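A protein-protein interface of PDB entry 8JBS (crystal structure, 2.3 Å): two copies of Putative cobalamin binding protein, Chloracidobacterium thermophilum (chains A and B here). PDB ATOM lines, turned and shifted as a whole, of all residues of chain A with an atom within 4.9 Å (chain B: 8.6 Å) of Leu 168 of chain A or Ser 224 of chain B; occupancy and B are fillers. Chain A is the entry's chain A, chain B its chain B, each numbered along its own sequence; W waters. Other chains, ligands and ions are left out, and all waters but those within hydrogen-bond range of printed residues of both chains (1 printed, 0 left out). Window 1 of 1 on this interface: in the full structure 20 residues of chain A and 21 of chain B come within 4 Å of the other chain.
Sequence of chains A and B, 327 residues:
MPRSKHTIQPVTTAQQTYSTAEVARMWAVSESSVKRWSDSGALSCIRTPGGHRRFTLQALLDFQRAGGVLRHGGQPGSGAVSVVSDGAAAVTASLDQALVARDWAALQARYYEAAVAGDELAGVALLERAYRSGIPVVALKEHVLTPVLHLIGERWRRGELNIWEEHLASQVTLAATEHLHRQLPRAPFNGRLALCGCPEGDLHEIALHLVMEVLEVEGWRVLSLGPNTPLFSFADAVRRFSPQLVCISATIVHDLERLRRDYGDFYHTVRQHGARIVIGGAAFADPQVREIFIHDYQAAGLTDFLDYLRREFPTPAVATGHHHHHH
No position is printed for both chains. Of the 17 pairs that touch across the chains among the printed residues, none has its exchanged pair printed and touching as well.
The backbone carbonyl oxygen (O) of Pro 227 of chain B is in hydrogen-bond range of a ring nitrogen (NE2) of His 167 of chain A, at 3.5 Å.
Among the printed residues, pairs that only touch across the chains: His 167 of chain A with Leu 225 of chain B (3.0 Å), Trp 164 of chain A with Asp 236 of chain B (3.2 Å), Gln 171 of chain A with Ser 224 of chain B (3.3 Å), Leu 168 of chain A with Ser 224 of chain B (3.3 Å), His 167 of chain A with Thr 229 of chain B (3.3 Å), Ala 117 of chain A with Phe 241 of chain B (3.4 Å), Gly 118 of chain A with Leu 223 of chain B (3.4 Å), Trp 164 of chain A with Phe 241 of chain B (3.4 Å), Trp 164 of chain A with Ser 233 of chain B (3.5 Å), Trp 164 of chain A with Leu 225 of chain B (3.5 Å), Leu 168 of chain A with Phe 241 of chain B (3.8 Å), Leu 168 of chain A with Leu 225 of chain B (3.9 Å), Gln 171 of chain A with Gly 226 of chain B (3.9 Å), Trp 164 of chain A with Arg 240 of chain B (3.9 Å), Ala 117 of chain A with Leu 223 of chain B (3.9 Å) and Ala 117 of chain A with Arg 240 of chain B (3.95 Å).
Of the printed residues of chain B, His 167 of chain A touches Leu 225, Pro 227 and Thr 229. Of chain B, only Ser 224, Leu 225 and Phe 241 come within 4 Å of Leu 168 of chain A. Ser 224 of chain B touches just these residues of chain A: Leu 168 (3.3 Å) and Gln 171 (3.3 Å). Of the printed residues of chain A, Gly 226 of chain B touches Gln 171. Of the printed residues of chain A, Arg 240 of chain B touches Ala 117 and Trp 164. The nearest residue of chain B that does not touch Leu 168 of chain A is Leu 223 of chain B (4.2 Å).
ND1 of His 167 of chain A sits at hydrogen-bond distance from OE1 of Glu 166 of chain A (2.6 Å). O of Leu 223 of chain B sits at hydrogen-bond distance from N of Cys 196 of chain B (2.8 Å). O of Cys 196 of chain B lies within hydrogen-bond range of N of Leu 225 of chain B, at 2.8 Å. The backbone carbonyl oxygen (O) of Gly 226 of chain B sits at hydrogen-bond distance from the backbone NH (N) of Cys 198 of chain B (3.2 Å). The side-chain sulfur of Met 212 of chain B lies within hydrogen-bond range of the side-chain hydroxyl of Ser 224 of chain B (3.3 Å). The backbone NH of Gly 226 of chain B sits close to the side-chain hydroxyl of Ser 224 of chain B (3.4 Å).
Water W1 bridges the backbone carbonyl oxygen (O) of Pro 227 of chain B (2.8 Å) and a ring nitrogen (NE2) of His 167 of chain A (3.4 Å).
Hydrophobic or aromatic side chains of chain B that line the printed part of chain A: Leu 223, Leu 225 and Phe 241. Among the printed residues, 17 pairs touch across the chains.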
ATOM      1  N   ALA A 115      13.722  -0.638  17.482  1.00  0.00           N
ATOM      2  CA  ALA A 115      13.913   0.167  16.289  1.00  0.00           C
ATOM      3  C   ALA A 115      15.070  -0.387  15.453  1.00  0.00           C
ATOM      4  O   ALA A 115      14.897  -0.712  14.273  1.00  0.00           O
ATOM      5  CB  ALA A 115      14.131   1.618  16.686  1.00  0.00           C
ATOM      6  N   VAL A 116      16.257  -0.519  16.060  1.00  0.00           N
ATOM      7  CA  VAL A 116      17.424  -0.953  15.299  1.00  0.00           C
ATOM      8  C   VAL A 116      17.240  -2.392  14.812  1.00  0.00           C
ATOM      9  O   VAL A 116      18.024  -2.856  13.993  1.00  0.00           O
ATOM     10  CB  VAL A 116      18.748  -0.809  16.073  1.00  0.00           C
ATOM     11  CG1 VAL A 116      18.993   0.634  16.520  1.00  0.00           C
ATOM     12  CG2 VAL A 116      18.815  -1.753  17.272  1.00  0.00           C
ATOM     13  N   ALA A 117      16.214  -3.106  15.289  1.00  0.00           N
ATOM     14  CA  ALA A 117      16.015  -4.482  14.869  1.00  0.00           C
ATOM     15  C   ALA A 117      14.932  -4.567  13.796  1.00  0.00           C
ATOM     16  O   ALA A 117      14.691  -5.643  13.250  1.00  0.00           O
ATOM     17  CB  ALA A 117      15.679  -5.344  16.075  1.00  0.00           C
ATOM     18  N   GLY A 118      14.265  -3.444  13.519  1.00  0.00           N
ATOM     19  CA  GLY A 118      13.256  -3.388  12.472  1.00  0.00           C
ATOM     20  C   GLY A 118      11.922  -3.930  12.978  1.00  0.00           C
ATOM     21  O   GLY A 118      11.089  -4.374  12.190  1.00  0.00           O
ATOM     22  N   TRP A 164      22.403   0.522   8.266  1.00  0.00           N
ATOM     23  CA  TRP A 164      21.245  -0.340   8.077  1.00  0.00           C
ATOM     24  C   TRP A 164      20.396  -0.301   9.334  1.00  0.00           C
ATOM     25  O   TRP A 164      19.191  -0.499   9.276  1.00  0.00           O
ATOM     26  CB  TRP A 164      21.635  -1.772   7.675  1.00  0.00           C
ATOM     27  CG  TRP A 164      22.429  -2.521   8.705  1.00  0.00           C
ATOM     28  CD1 TRP A 164      23.787  -2.534   8.838  1.00  0.00           C
ATOM     29  CD2 TRP A 164      21.904  -3.360   9.756  1.00  0.00           C
ATOM     30  NE1 TRP A 164      24.150  -3.317   9.901  1.00  0.00           N
ATOM     31  CE2 TRP A 164      23.019  -3.840  10.483  1.00  0.00           C
ATOM     32  CE3 TRP A 164      20.619  -3.753  10.154  1.00  0.00           C
ATOM     33  CZ2 TRP A 164      22.874  -4.685  11.584  1.00  0.00           C
ATOM     34  CZ3 TRP A 164      20.480  -4.592  11.242  1.00  0.00           C
ATOM     35  CH2 TRP A 164      21.593  -5.043  11.950  1.00  0.00           C
ATOM     36  N   GLU A 165      21.022   0.022  10.464  1.00  0.00           N
ATOM     37  CA  GLU A 165      20.315  -0.017  11.732  1.00  0.00           C
ATOM     38  C   GLU A 165      19.522   1.279  11.923  1.00  0.00           C
ATOM     39  O   GLU A 165      18.460   1.303  12.536  1.00  0.00           O
ATOM     40  CB  GLU A 165      21.326  -0.247  12.860  1.00  0.00           C
ATOM     41  CG  GLU A 165      22.148  -1.538  12.768  1.00  0.00           C
ATOM     42  CD  GLU A 165      23.286  -1.582  13.784  1.00  0.00           C
ATOM     43  OE1 GLU A 165      22.990  -1.768  14.971  1.00  0.00           O
ATOM     44  OE2 GLU A 165      24.455  -1.359  13.425  1.00  0.00           O
ATOM     45  N   GLU A 166      20.068   2.388  11.422  1.00  0.00           N
ATOM     46  CA  GLU A 166      19.379   3.668  11.481  1.00  0.00           C
ATOM     47  C   GLU A 166      18.167   3.608  10.553  1.00  0.00           C
ATOM     48  O   GLU A 166      17.065   3.947  10.972  1.00  0.00           O
ATOM     49  CB  GLU A 166      20.372   4.790  11.167  1.00  0.00           C
ATOM     50  CG  GLU A 166      19.706   6.099  10.775  1.00  0.00           C
ATOM     51  CD  GLU A 166      19.167   6.063   9.366  1.00  0.00           C
ATOM     52  OE1 GLU A 166      19.977   5.820   8.437  1.00  0.00           O
ATOM     53  OE2 GLU A 166      17.940   6.311   9.219  1.00  0.00           O
ATOM     54  N   HIS A 167      18.388   3.121   9.321  1.00  0.00           N
ATOM     55  CA  HIS A 167      17.349   3.004   8.307  1.00  0.00           C
ATOM     56  C   HIS A 167      16.145   2.219   8.822  1.00  0.00           C
ATOM     57  O   HIS A 167      15.018   2.584   8.513  1.00  0.00           O
ATOM     58  CB  HIS A 167      17.883   2.392   6.999  1.00  0.00           C
ATOM     59  CG  HIS A 167      18.473   3.358   6.029  1.00  0.00           C
ATOM     60  ND1 HIS A 167      19.263   4.440   6.396  1.00  0.00           N
ATOM     61  CD2 HIS A 167      18.416   3.364   4.676  1.00  0.00           C
ATOM     62  CE1 HIS A 167      19.688   5.053   5.296  1.00  0.00           C
ATOM     63  NE2 HIS A 167      19.176   4.428   4.234  1.00  0.00           N
ATOM     64  N   LEU A 168      16.374   1.137   9.579  1.00  0.00           N
ATOM     65  CA  LEU A 168      15.272   0.351  10.124  1.00  0.00           C
ATOM     66  C   LEU A 168      14.569   1.148  11.222  1.00  0.00           C
ATOM     67  O   LEU A 168      13.343   1.192  11.283  1.00  0.00           O
ATOM     68  CB  LEU A 168      15.794  -0.978  10.658  1.00  0.00           C
ATOM     69  CG  LEU A 168      16.232  -2.002   9.616  1.00  0.00           C
ATOM     70  CD1 LEU A 168      16.904  -3.134  10.352  1.00  0.00           C
ATOM     71  CD2 LEU A 168      15.052  -2.485   8.786  1.00  0.00           C
ATOM     72  N   ALA A 169      15.366   1.776  12.091  1.00  0.00           N
ATOM     73  CA  ALA A 169      14.849   2.604  13.162  1.00  0.00           C
ATOM     74  C   ALA A 169      13.973   3.728  12.605  1.00  0.00           C
ATOM     75  O   ALA A 169      12.870   3.994  13.109  1.00  0.00           O
ATOM     76  CB  ALA A 169      16.018   3.144  13.970  1.00  0.00           C
ATOM     77  N   SER A 170      14.472   4.386  11.550  1.00  0.00           N
ATOM     78  CA  SER A 170      13.710   5.421  10.863  1.00  0.00           C
ATOM     79  C   SER A 170      12.374   4.869  10.352  1.00  0.00           C
ATOM     80  O   SER A 170      11.325   5.424  10.657  1.00  0.00           O
ATOM     81  CB  SER A 170      14.532   6.069   9.774  1.00  0.00           C
ATOM     82  OG  SER A 170      15.572   6.868  10.339  1.00  0.00           O
ATOM     83  N   GLN A 171      12.372   3.745   9.623  1.00  0.00           N
ATOM     84  CA  GLN A 171      11.108   3.198   9.130  1.00  0.00           C
ATOM     85  C   GLN A 171      10.186   2.786  10.275  1.00  0.00           C
ATOM     86  O   GLN A 171       8.992   3.083  10.226  1.00  0.00           O
ATOM     87  CB  GLN A 171      11.273   1.969   8.247  1.00  0.00           C
ATOM     88  CG  GLN A 171      11.965   2.262   6.928  1.00  0.00           C
ATOM     89  CD  GLN A 171      11.289   3.377   6.165  1.00  0.00           C
ATOM     90  OE1 GLN A 171      10.136   3.256   5.742  1.00  0.00           O
ATOM     91  NE2 GLN A 171      12.023   4.457   5.944  1.00  0.00           N
ATOM     92  N   VAL A 172      10.735   2.113  11.299  1.00  0.00           N
ATOM     93  CA  VAL A 172       9.941   1.715  12.457  1.00  0.00           C
ATOM     94  C   VAL A 172       9.275   2.948  13.072  1.00  0.00           C
ATOM     95  O   VAL A 172       8.071   2.929  13.335  1.00  0.00           O
ATOM     96  CB  VAL A 172      10.755   0.937  13.514  1.00  0.00           C
ATOM     97  CG1 VAL A 172      10.046   0.899  14.861  1.00  0.00           C
ATOM     98  CG2 VAL A 172      11.104  -0.486  13.051  1.00  0.00           C
ATOM     99  N   THR A 173      10.050   4.018  13.291  1.00  0.00           N
ATOM    100  CA  THR A 173       9.551   5.167  14.028  1.00  0.00           C
ATOM    101  C   THR A 173       8.451   5.885  13.237  1.00  0.00           C
ATOM    102  O   THR A 173       7.496   6.377  13.824  1.00  0.00           O
ATOM    103  CB  THR A 173      10.687   6.129  14.381  1.00  0.00           C
ATOM    104  OG1 THR A 173      11.720   5.423  15.066  1.00  0.00           O
ATOM    105  CG2 THR A 173      10.185   7.290  15.221  1.00  0.00           C
ATOM    106  N   LEU B 193      10.372 -14.027   5.035  1.00  0.00           N
ATOM    107  CA  LEU B 193      10.788 -12.657   5.289  1.00  0.00           C
ATOM    108  C   LEU B 193      11.335 -12.035   4.004  1.00  0.00           C
ATOM    109  O   LEU B 193      12.255 -12.585   3.400  1.00  0.00           O
ATOM    110  CB  LEU B 193      11.843 -12.640   6.392  1.00  0.00           C
ATOM    111  CG  LEU B 193      12.434 -11.275   6.758  1.00  0.00           C
ATOM    112  CD1 LEU B 193      11.366 -10.391   7.324  1.00  0.00           C
ATOM    113  CD2 LEU B 193      13.593 -11.408   7.737  1.00  0.00           C
ATOM    114  N   ALA B 194      10.774 -10.867   3.648  1.00  0.00           N
ATOM    115  CA  ALA B 194      11.246 -10.024   2.554  1.00  0.00           C
ATOM    116  C   ALA B 194      11.960  -8.790   3.100  1.00  0.00           C
ATOM    117  O   ALA B 194      11.421  -8.101   3.981  1.00  0.00           O
ATOM    118  CB  ALA B 194      10.084  -9.598   1.702  1.00  0.00           C
ATOM    119  N   LEU B 195      13.158  -8.532   2.542  1.00  0.00           N
ATOM    120  CA  LEU B 195      13.961  -7.342   2.828  1.00  0.00           C
ATOM    121  C   LEU B 195      13.871  -6.344   1.669  1.00  0.00           C
ATOM    122  O   LEU B 195      14.268  -6.690   0.553  1.00  0.00           O
ATOM    123  CB  LEU B 195      15.411  -7.773   3.031  1.00  0.00           C
ATOM    124  CG  LEU B 195      16.368  -6.640   3.388  1.00  0.00           C
ATOM    125  CD1 LEU B 195      16.076  -6.072   4.777  1.00  0.00           C
ATOM    126  CD2 LEU B 195      17.774  -7.130   3.279  1.00  0.00           C
ATOM    127  N   CYS B 196      13.403  -5.110   1.939  1.00  0.00           N
ATOM    128  CA  CYS B 196      13.042  -4.173   0.872  1.00  0.00           C
ATOM    129  C   CYS B 196      13.741  -2.815   1.005  1.00  0.00           C
ATOM    130  O   CYS B 196      13.960  -2.284   2.107  1.00  0.00           O
ATOM    131  CB  CYS B 196      11.533  -4.034   0.787  1.00  0.00           C
ATOM    132  SG  CYS B 196      10.704  -5.626   0.520  1.00  0.00           S
ATOM    133  N   GLY B 197      14.132  -2.267  -0.157  1.00  0.00           N
ATOM    134  CA  GLY B 197      14.864  -1.009  -0.204  1.00  0.00           C
ATOM    135  C   GLY B 197      14.936  -0.404  -1.608  1.00  0.00           C
ATOM    136  O   GLY B 197      14.552  -1.017  -2.605  1.00  0.00           O
ATOM    137  N   CYS B 198      15.437   0.836  -1.670  1.00  0.00           N
ATOM    138  CA  CYS B 198      15.827   1.447  -2.929  1.00  0.00           C
ATOM    139  C   CYS B 198      17.304   1.793  -2.840  1.00  0.00           C
ATOM    140  O   CYS B 198      17.825   1.979  -1.733  1.00  0.00           O
ATOM    141  CB  CYS B 198      15.033   2.714  -3.177  1.00  0.00           C
ATOM    142  SG  CYS B 198      13.260   2.560  -2.854  1.00  0.00           S
ATOM    143  N   GLU B 205      10.206   6.362  -3.461  1.00  0.00           N
ATOM    144  CA  GLU B 205       9.953   5.284  -2.523  1.00  0.00           C
ATOM    145  C   GLU B 205       8.504   4.836  -2.554  1.00  0.00           C
ATOM    146  O   GLU B 205       8.177   3.927  -1.802  1.00  0.00           O
ATOM    147  CB  GLU B 205      10.381   5.574  -1.080  1.00  0.00           C
ATOM    148  CG  GLU B 205       9.443   6.486  -0.289  1.00  0.00           C
ATOM    149  CD  GLU B 205      10.054   7.076   0.977  1.00  0.00           C
ATOM    150  OE1 GLU B 205      10.369   6.313   1.936  1.00  0.00           O
ATOM    151  OE2 GLU B 205      10.196   8.327   0.991  1.00  0.00           O
ATOM    152  N   LEU B 208       8.114   1.119  -3.765  1.00  0.00           N
ATOM    153  CA  LEU B 208       8.576   0.218  -2.733  1.00  0.00           C
ATOM    154  C   LEU B 208       7.438  -0.015  -1.739  1.00  0.00           C
ATOM    155  O   LEU B 208       7.232  -1.130  -1.281  1.00  0.00           O
ATOM    156  CB  LEU B 208       9.799   0.814  -2.043  1.00  0.00           C
ATOM    157  CG  LEU B 208      10.497  -0.097  -1.025  1.00  0.00           C
ATOM    158  CD1 LEU B 208      11.276  -1.205  -1.726  1.00  0.00           C
ATOM    159  CD2 LEU B 208      11.444   0.686  -0.126  1.00  0.00           C
ATOM    160  N   HIS B 209       6.695   1.040  -1.400  1.00  0.00           N
ATOM    161  CA  HIS B 209       5.599   0.900  -0.452  1.00  0.00           C
ATOM    162  C   HIS B 209       4.542  -0.012  -1.059  1.00  0.00           C
ATOM    163  O   HIS B 209       3.955  -0.806  -0.343  1.00  0.00           O
ATOM    164  CB  HIS B 209       5.016   2.256  -0.003  1.00  0.00           C
ATOM    165  CG  HIS B 209       5.828   2.902   1.070  1.00  0.00           C
ATOM    166  ND1 HIS B 209       7.118   3.345   0.865  1.00  0.00           N
ATOM    167  CD2 HIS B 209       5.574   3.081   2.360  1.00  0.00           C
ATOM    168  CE1 HIS B 209       7.613   3.803   2.006  1.00  0.00           C
ATOM    169  NE2 HIS B 209       6.683   3.646   2.930  1.00  0.00           N
ATOM    170  N   MET B 212       5.824  -3.730  -0.866  1.00  0.00           N
ATOM    171  CA  MET B 212       5.856  -4.173   0.514  1.00  0.00           C
ATOM    172  C   MET B 212       4.432  -4.467   0.987  1.00  0.00           C
ATOM    173  O   MET B 212       4.165  -5.478   1.623  1.00  0.00           O
ATOM    174  CB  MET B 212       6.534  -3.119   1.400  1.00  0.00           C
ATOM    175  CG  MET B 212       8.043  -2.991   1.181  1.00  0.00           C
ATOM    176  SD  MET B 212       8.886  -1.962   2.411  1.00  0.00           S
ATOM    177  CE  MET B 212       8.013  -0.420   2.137  1.00  0.00           C
ATOM    178  N   GLU B 216       2.816  -8.115   2.353  1.00  0.00           N
ATOM    179  CA  GLU B 216       2.165  -8.361   3.633  1.00  0.00           C
ATOM    180  C   GLU B 216       0.763  -8.963   3.471  1.00  0.00           C
ATOM    181  O   GLU B 216       0.348  -9.780   4.291  1.00  0.00           O
ATOM    182  CB  GLU B 216       2.106  -7.060   4.430  1.00  0.00           C
ATOM    183  CG  GLU B 216       3.457  -6.647   5.001  1.00  0.00           C
ATOM    184  CD  GLU B 216       3.318  -5.425   5.888  1.00  0.00           C
ATOM    185  OE1 GLU B 216       2.272  -4.746   5.777  1.00  0.00           O
ATOM    186  OE2 GLU B 216       4.229  -5.160   6.698  1.00  0.00           O
ATOM    187  N   ARG B 221       6.294 -11.307   6.127  1.00  0.00           N
ATOM    188  CA  ARG B 221       6.789 -10.289   7.031  1.00  0.00           C
ATOM    189  C   ARG B 221       7.840  -9.538   6.227  1.00  0.00           C
ATOM    190  O   ARG B 221       8.508 -10.150   5.405  1.00  0.00           O
ATOM    191  CB  ARG B 221       7.284 -10.889   8.357  1.00  0.00           C
ATOM    192  CG  ARG B 221       7.937  -9.918   9.334  1.00  0.00           C
ATOM    193  CD  ARG B 221       8.497 -10.632  10.560  1.00  0.00           C
ATOM    194  NE  ARG B 221       9.648  -9.925  11.146  1.00  0.00           N
ATOM    195  CZ  ARG B 221      10.781 -10.485  11.597  1.00  0.00           C
ATOM    196  NH1 ARG B 221      10.901 -11.803  11.658  1.00  0.00           N
ATOM    197  NH2 ARG B 221      11.782  -9.724  12.020  1.00  0.00           N
ATOM    198  N   VAL B 222       7.929  -8.219   6.431  1.00  0.00           N
ATOM    199  CA  VAL B 222       8.716  -7.350   5.575  1.00  0.00           C
ATOM    200  C   VAL B 222       9.650  -6.513   6.443  1.00  0.00           C
ATOM    201  O   VAL B 222       9.189  -5.894   7.376  1.00  0.00           O
ATOM    202  CB  VAL B 222       7.740  -6.463   4.788  1.00  0.00           C
ATOM    203  CG1 VAL B 222       8.464  -5.338   4.065  1.00  0.00           C
ATOM    204  CG2 VAL B 222       6.912  -7.262   3.800  1.00  0.00           C
ATOM    205  N   LEU B 223      10.950  -6.505   6.159  1.00  0.00           N
ATOM    206  CA  LEU B 223      11.850  -5.528   6.753  1.00  0.00           C
ATOM    207  C   LEU B 223      12.149  -4.455   5.709  1.00  0.00           C
ATOM    208  O   LEU B 223      12.654  -4.762   4.633  1.00  0.00           O
ATOM    209  CB  LEU B 223      13.156  -6.146   7.238  1.00  0.00           C
ATOM    210  CG  LEU B 223      13.126  -6.861   8.590  1.00  0.00           C
ATOM    211  CD1 LEU B 223      14.467  -7.543   8.744  1.00  0.00           C
ATOM    212  CD2 LEU B 223      12.881  -5.935   9.766  1.00  0.00           C
ATOM    213  N   SER B 224      11.835  -3.201   6.055  1.00  0.00           N
ATOM    214  CA  SER B 224      12.000  -2.055   5.174  1.00  0.00           C
ATOM    215  C   SER B 224      13.237  -1.271   5.584  1.00  0.00           C
ATOM    216  O   SER B 224      13.262  -0.712   6.682  1.00  0.00           O
ATOM    217  CB  SER B 224      10.795  -1.156   5.208  1.00  0.00           C
ATOM    218  OG  SER B 224      10.959  -0.130   4.244  1.00  0.00           O
ATOM    219  N   LEU B 225      14.239  -1.226   4.686  1.00  0.00           N
ATOM    220  CA  LEU B 225      15.382  -0.333   4.852  1.00  0.00           C
ATOM    221  C   LEU B 225      15.070   1.066   4.316  1.00  0.00           C
ATOM    222  O   LEU B 225      15.753   2.030   4.666  1.00  0.00           O
ATOM    223  CB  LEU B 225      16.609  -0.933   4.179  1.00  0.00           C
ATOM    224  CG  LEU B 225      17.272  -2.087   4.931  1.00  0.00           C
ATOM    225  CD1 LEU B 225      18.229  -2.777   4.010  1.00  0.00           C
ATOM    226  CD2 LEU B 225      17.973  -1.598   6.165  1.00  0.00           C
ATOM    227  N   GLY B 226      13.986   1.174   3.536  1.00  0.00           N
ATOM    228  CA  GLY B 226      13.575   2.439   2.964  1.00  0.00           C
ATOM    229  C   GLY B 226      14.464   2.806   1.772  1.00  0.00           C
ATOM    230  O   GLY B 226      15.290   2.011   1.309  1.00  0.00           O
ATOM    231  N   PRO B 227      14.320   4.038   1.240  1.00  0.00           N
ATOM    232  CA  PRO B 227      15.122   4.482   0.096  1.00  0.00           C
ATOM    233  C   PRO B 227      16.533   4.817   0.554  1.00  0.00           C
ATOM    234  O   PRO B 227      16.815   4.893   1.761  1.00  0.00           O
ATOM    235  CB  PRO B 227      14.350   5.734  -0.415  1.00  0.00           C
ATOM    236  CG  PRO B 227      13.618   6.254   0.809  1.00  0.00           C
ATOM    237  CD  PRO B 227      13.382   5.068   1.731  1.00  0.00           C
ATOM    238  N   THR B 229      19.472   3.349   0.351  1.00  0.00           N
ATOM    239  CA  THR B 229      20.146   2.264   1.061  1.00  0.00           C
ATOM    240  C   THR B 229      21.387   1.831   0.285  1.00  0.00           C
ATOM    241  O   THR B 229      21.279   1.234  -0.790  1.00  0.00           O
ATOM    242  CB  THR B 229      19.183   1.092   1.223  1.00  0.00           C
ATOM    243  OG1 THR B 229      18.043   1.580   1.920  1.00  0.00           O
ATOM    244  CG2 THR B 229      19.791  -0.039   2.021  1.00  0.00           C
ATOM    245  N   SER B 233      24.764  -1.931   2.683  1.00  0.00           N
ATOM    246  CA  SER B 233      23.868  -1.870   3.821  1.00  0.00           C
ATOM    247  C   SER B 233      22.765  -2.912   3.661  1.00  0.00           C
ATOM    248  O   SER B 233      22.267  -3.429   4.649  1.00  0.00           O
ATOM    249  CB  SER B 233      23.370  -0.464   4.055  1.00  0.00           C
ATOM    250  OG  SER B 233      24.394   0.279   4.705  1.00  0.00           O
ATOM    251  N   PHE B 234      22.409  -3.256   2.421  1.00  0.00           N
ATOM    252  CA  PHE B 234      21.517  -4.385   2.189  1.00  0.00           C
ATOM    253  C   PHE B 234      22.174  -5.686   2.664  1.00  0.00           C
ATOM    254  O   PHE B 234      21.530  -6.467   3.362  1.00  0.00           O
ATOM    255  CB  PHE B 234      21.137  -4.620   0.724  1.00  0.00           C
ATOM    256  CG  PHE B 234      20.016  -3.771   0.144  1.00  0.00           C
ATOM    257  CD1 PHE B 234      20.265  -2.482  -0.342  1.00  0.00           C
ATOM    258  CD2 PHE B 234      18.736  -4.301  -0.009  1.00  0.00           C
ATOM    259  CE1 PHE B 234      19.248  -1.742  -0.925  1.00  0.00           C
ATOM    260  CE2 PHE B 234      17.724  -3.550  -0.594  1.00  0.00           C
ATOM    261  CZ  PHE B 234      17.984  -2.278  -1.052  1.00  0.00           C
ATOM    262  N   ASP B 236      24.647  -6.134   4.836  1.00  0.00           N
ATOM    263  CA  ASP B 236      24.746  -6.178   6.279  1.00  0.00           C
ATOM    264  C   ASP B 236      23.476  -6.833   6.805  1.00  0.00           C
ATOM    265  O   ASP B 236      23.541  -7.744   7.624  1.00  0.00           O
ATOM    266  CB  ASP B 236      24.949  -4.803   6.892  1.00  0.00           C
ATOM    267  CG  ASP B 236      26.294  -4.147   6.622  1.00  0.00           C
ATOM    268  OD1 ASP B 236      27.225  -4.890   6.268  1.00  0.00           O
ATOM    269  OD2 ASP B 236      26.393  -2.898   6.760  1.00  0.00           O
ATOM    270  N   ALA B 237      22.329  -6.374   6.301  1.00  0.00           N
ATOM    271  CA  ALA B 237      21.049  -6.765   6.861  1.00  0.00           C
ATOM    272  C   ALA B 237      20.669  -8.191   6.465  1.00  0.00           C
ATOM    273  O   ALA B 237      19.862  -8.809   7.149  1.00  0.00           O
ATOM    274  CB  ALA B 237      19.971  -5.802   6.418  1.00  0.00           C
ATOM    275  N   ARG B 240      22.209 -10.620   9.002  1.00  0.00           N
ATOM    276  CA  ARG B 240      21.230 -10.796  10.099  1.00  0.00           C
ATOM    277  C   ARG B 240      19.905 -11.118   9.417  1.00  0.00           C
ATOM    278  O   ARG B 240      19.912 -11.206   8.199  1.00  0.00           O
ATOM    279  CB  ARG B 240      21.085  -9.498  10.892  1.00  0.00           C
ATOM    280  CG  ARG B 240      21.164  -9.666  12.401  1.00  0.00           C
ATOM    281  CD  ARG B 240      20.373  -8.592  13.123  1.00  0.00           C
ATOM    282  NE  ARG B 240      19.359  -9.167  14.012  1.00  0.00           N
ATOM    283  CZ  ARG B 240      18.643  -8.468  14.881  1.00  0.00           C
ATOM    284  NH1 ARG B 240      17.534  -8.976  15.383  1.00  0.00           N
ATOM    285  NH2 ARG B 240      19.036  -7.261  15.241  1.00  0.00           N
ATOM    286  N   PHE B 241      18.834 -11.368  10.152  1.00  0.00           N
ATOM    287  CA  PHE B 241      17.491 -11.534   9.523  1.00  0.00           C
ATOM    288  C   PHE B 241      17.400 -12.739   8.567  1.00  0.00           C
ATOM    289  O   PHE B 241      16.338 -13.377   8.551  1.00  0.00           O
ATOM    290  CB  PHE B 241      17.152 -10.191   8.871  1.00  0.00           C
ATOM    291  CG  PHE B 241      17.265  -9.008   9.822  1.00  0.00           C
ATOM    292  CD1 PHE B 241      16.676  -9.047  11.079  1.00  0.00           C
ATOM    293  CD2 PHE B 241      17.956  -7.862   9.456  1.00  0.00           C
ATOM    294  CE1 PHE B 241      16.776  -7.967  11.938  1.00  0.00           C
ATOM    295  CE2 PHE B 241      18.052  -6.788  10.321  1.00  0.00           C
ATOM    296  CZ  PHE B 241      17.464  -6.843  11.559  1.00  0.00           C
ATOM    297  N   CYS B 247      13.999  -7.438  -2.196  1.00  0.00           N
ATOM    298  CA  CYS B 247      13.336  -6.638  -3.221  1.00  0.00           C
ATOM    299  C   CYS B 247      14.023  -5.281  -3.366  1.00  0.00           C
ATOM    300  O   CYS B 247      14.363  -4.655  -2.372  1.00  0.00           O
ATOM    301  CB  CYS B 247      11.891  -6.370  -2.841  1.00  0.00           C
ATOM    302  SG  CYS B 247      10.851  -7.840  -2.942  1.00  0.00           S
HETATM  303  O   HOH W   1      16.564   6.517   4.006  1.00  0.00           O
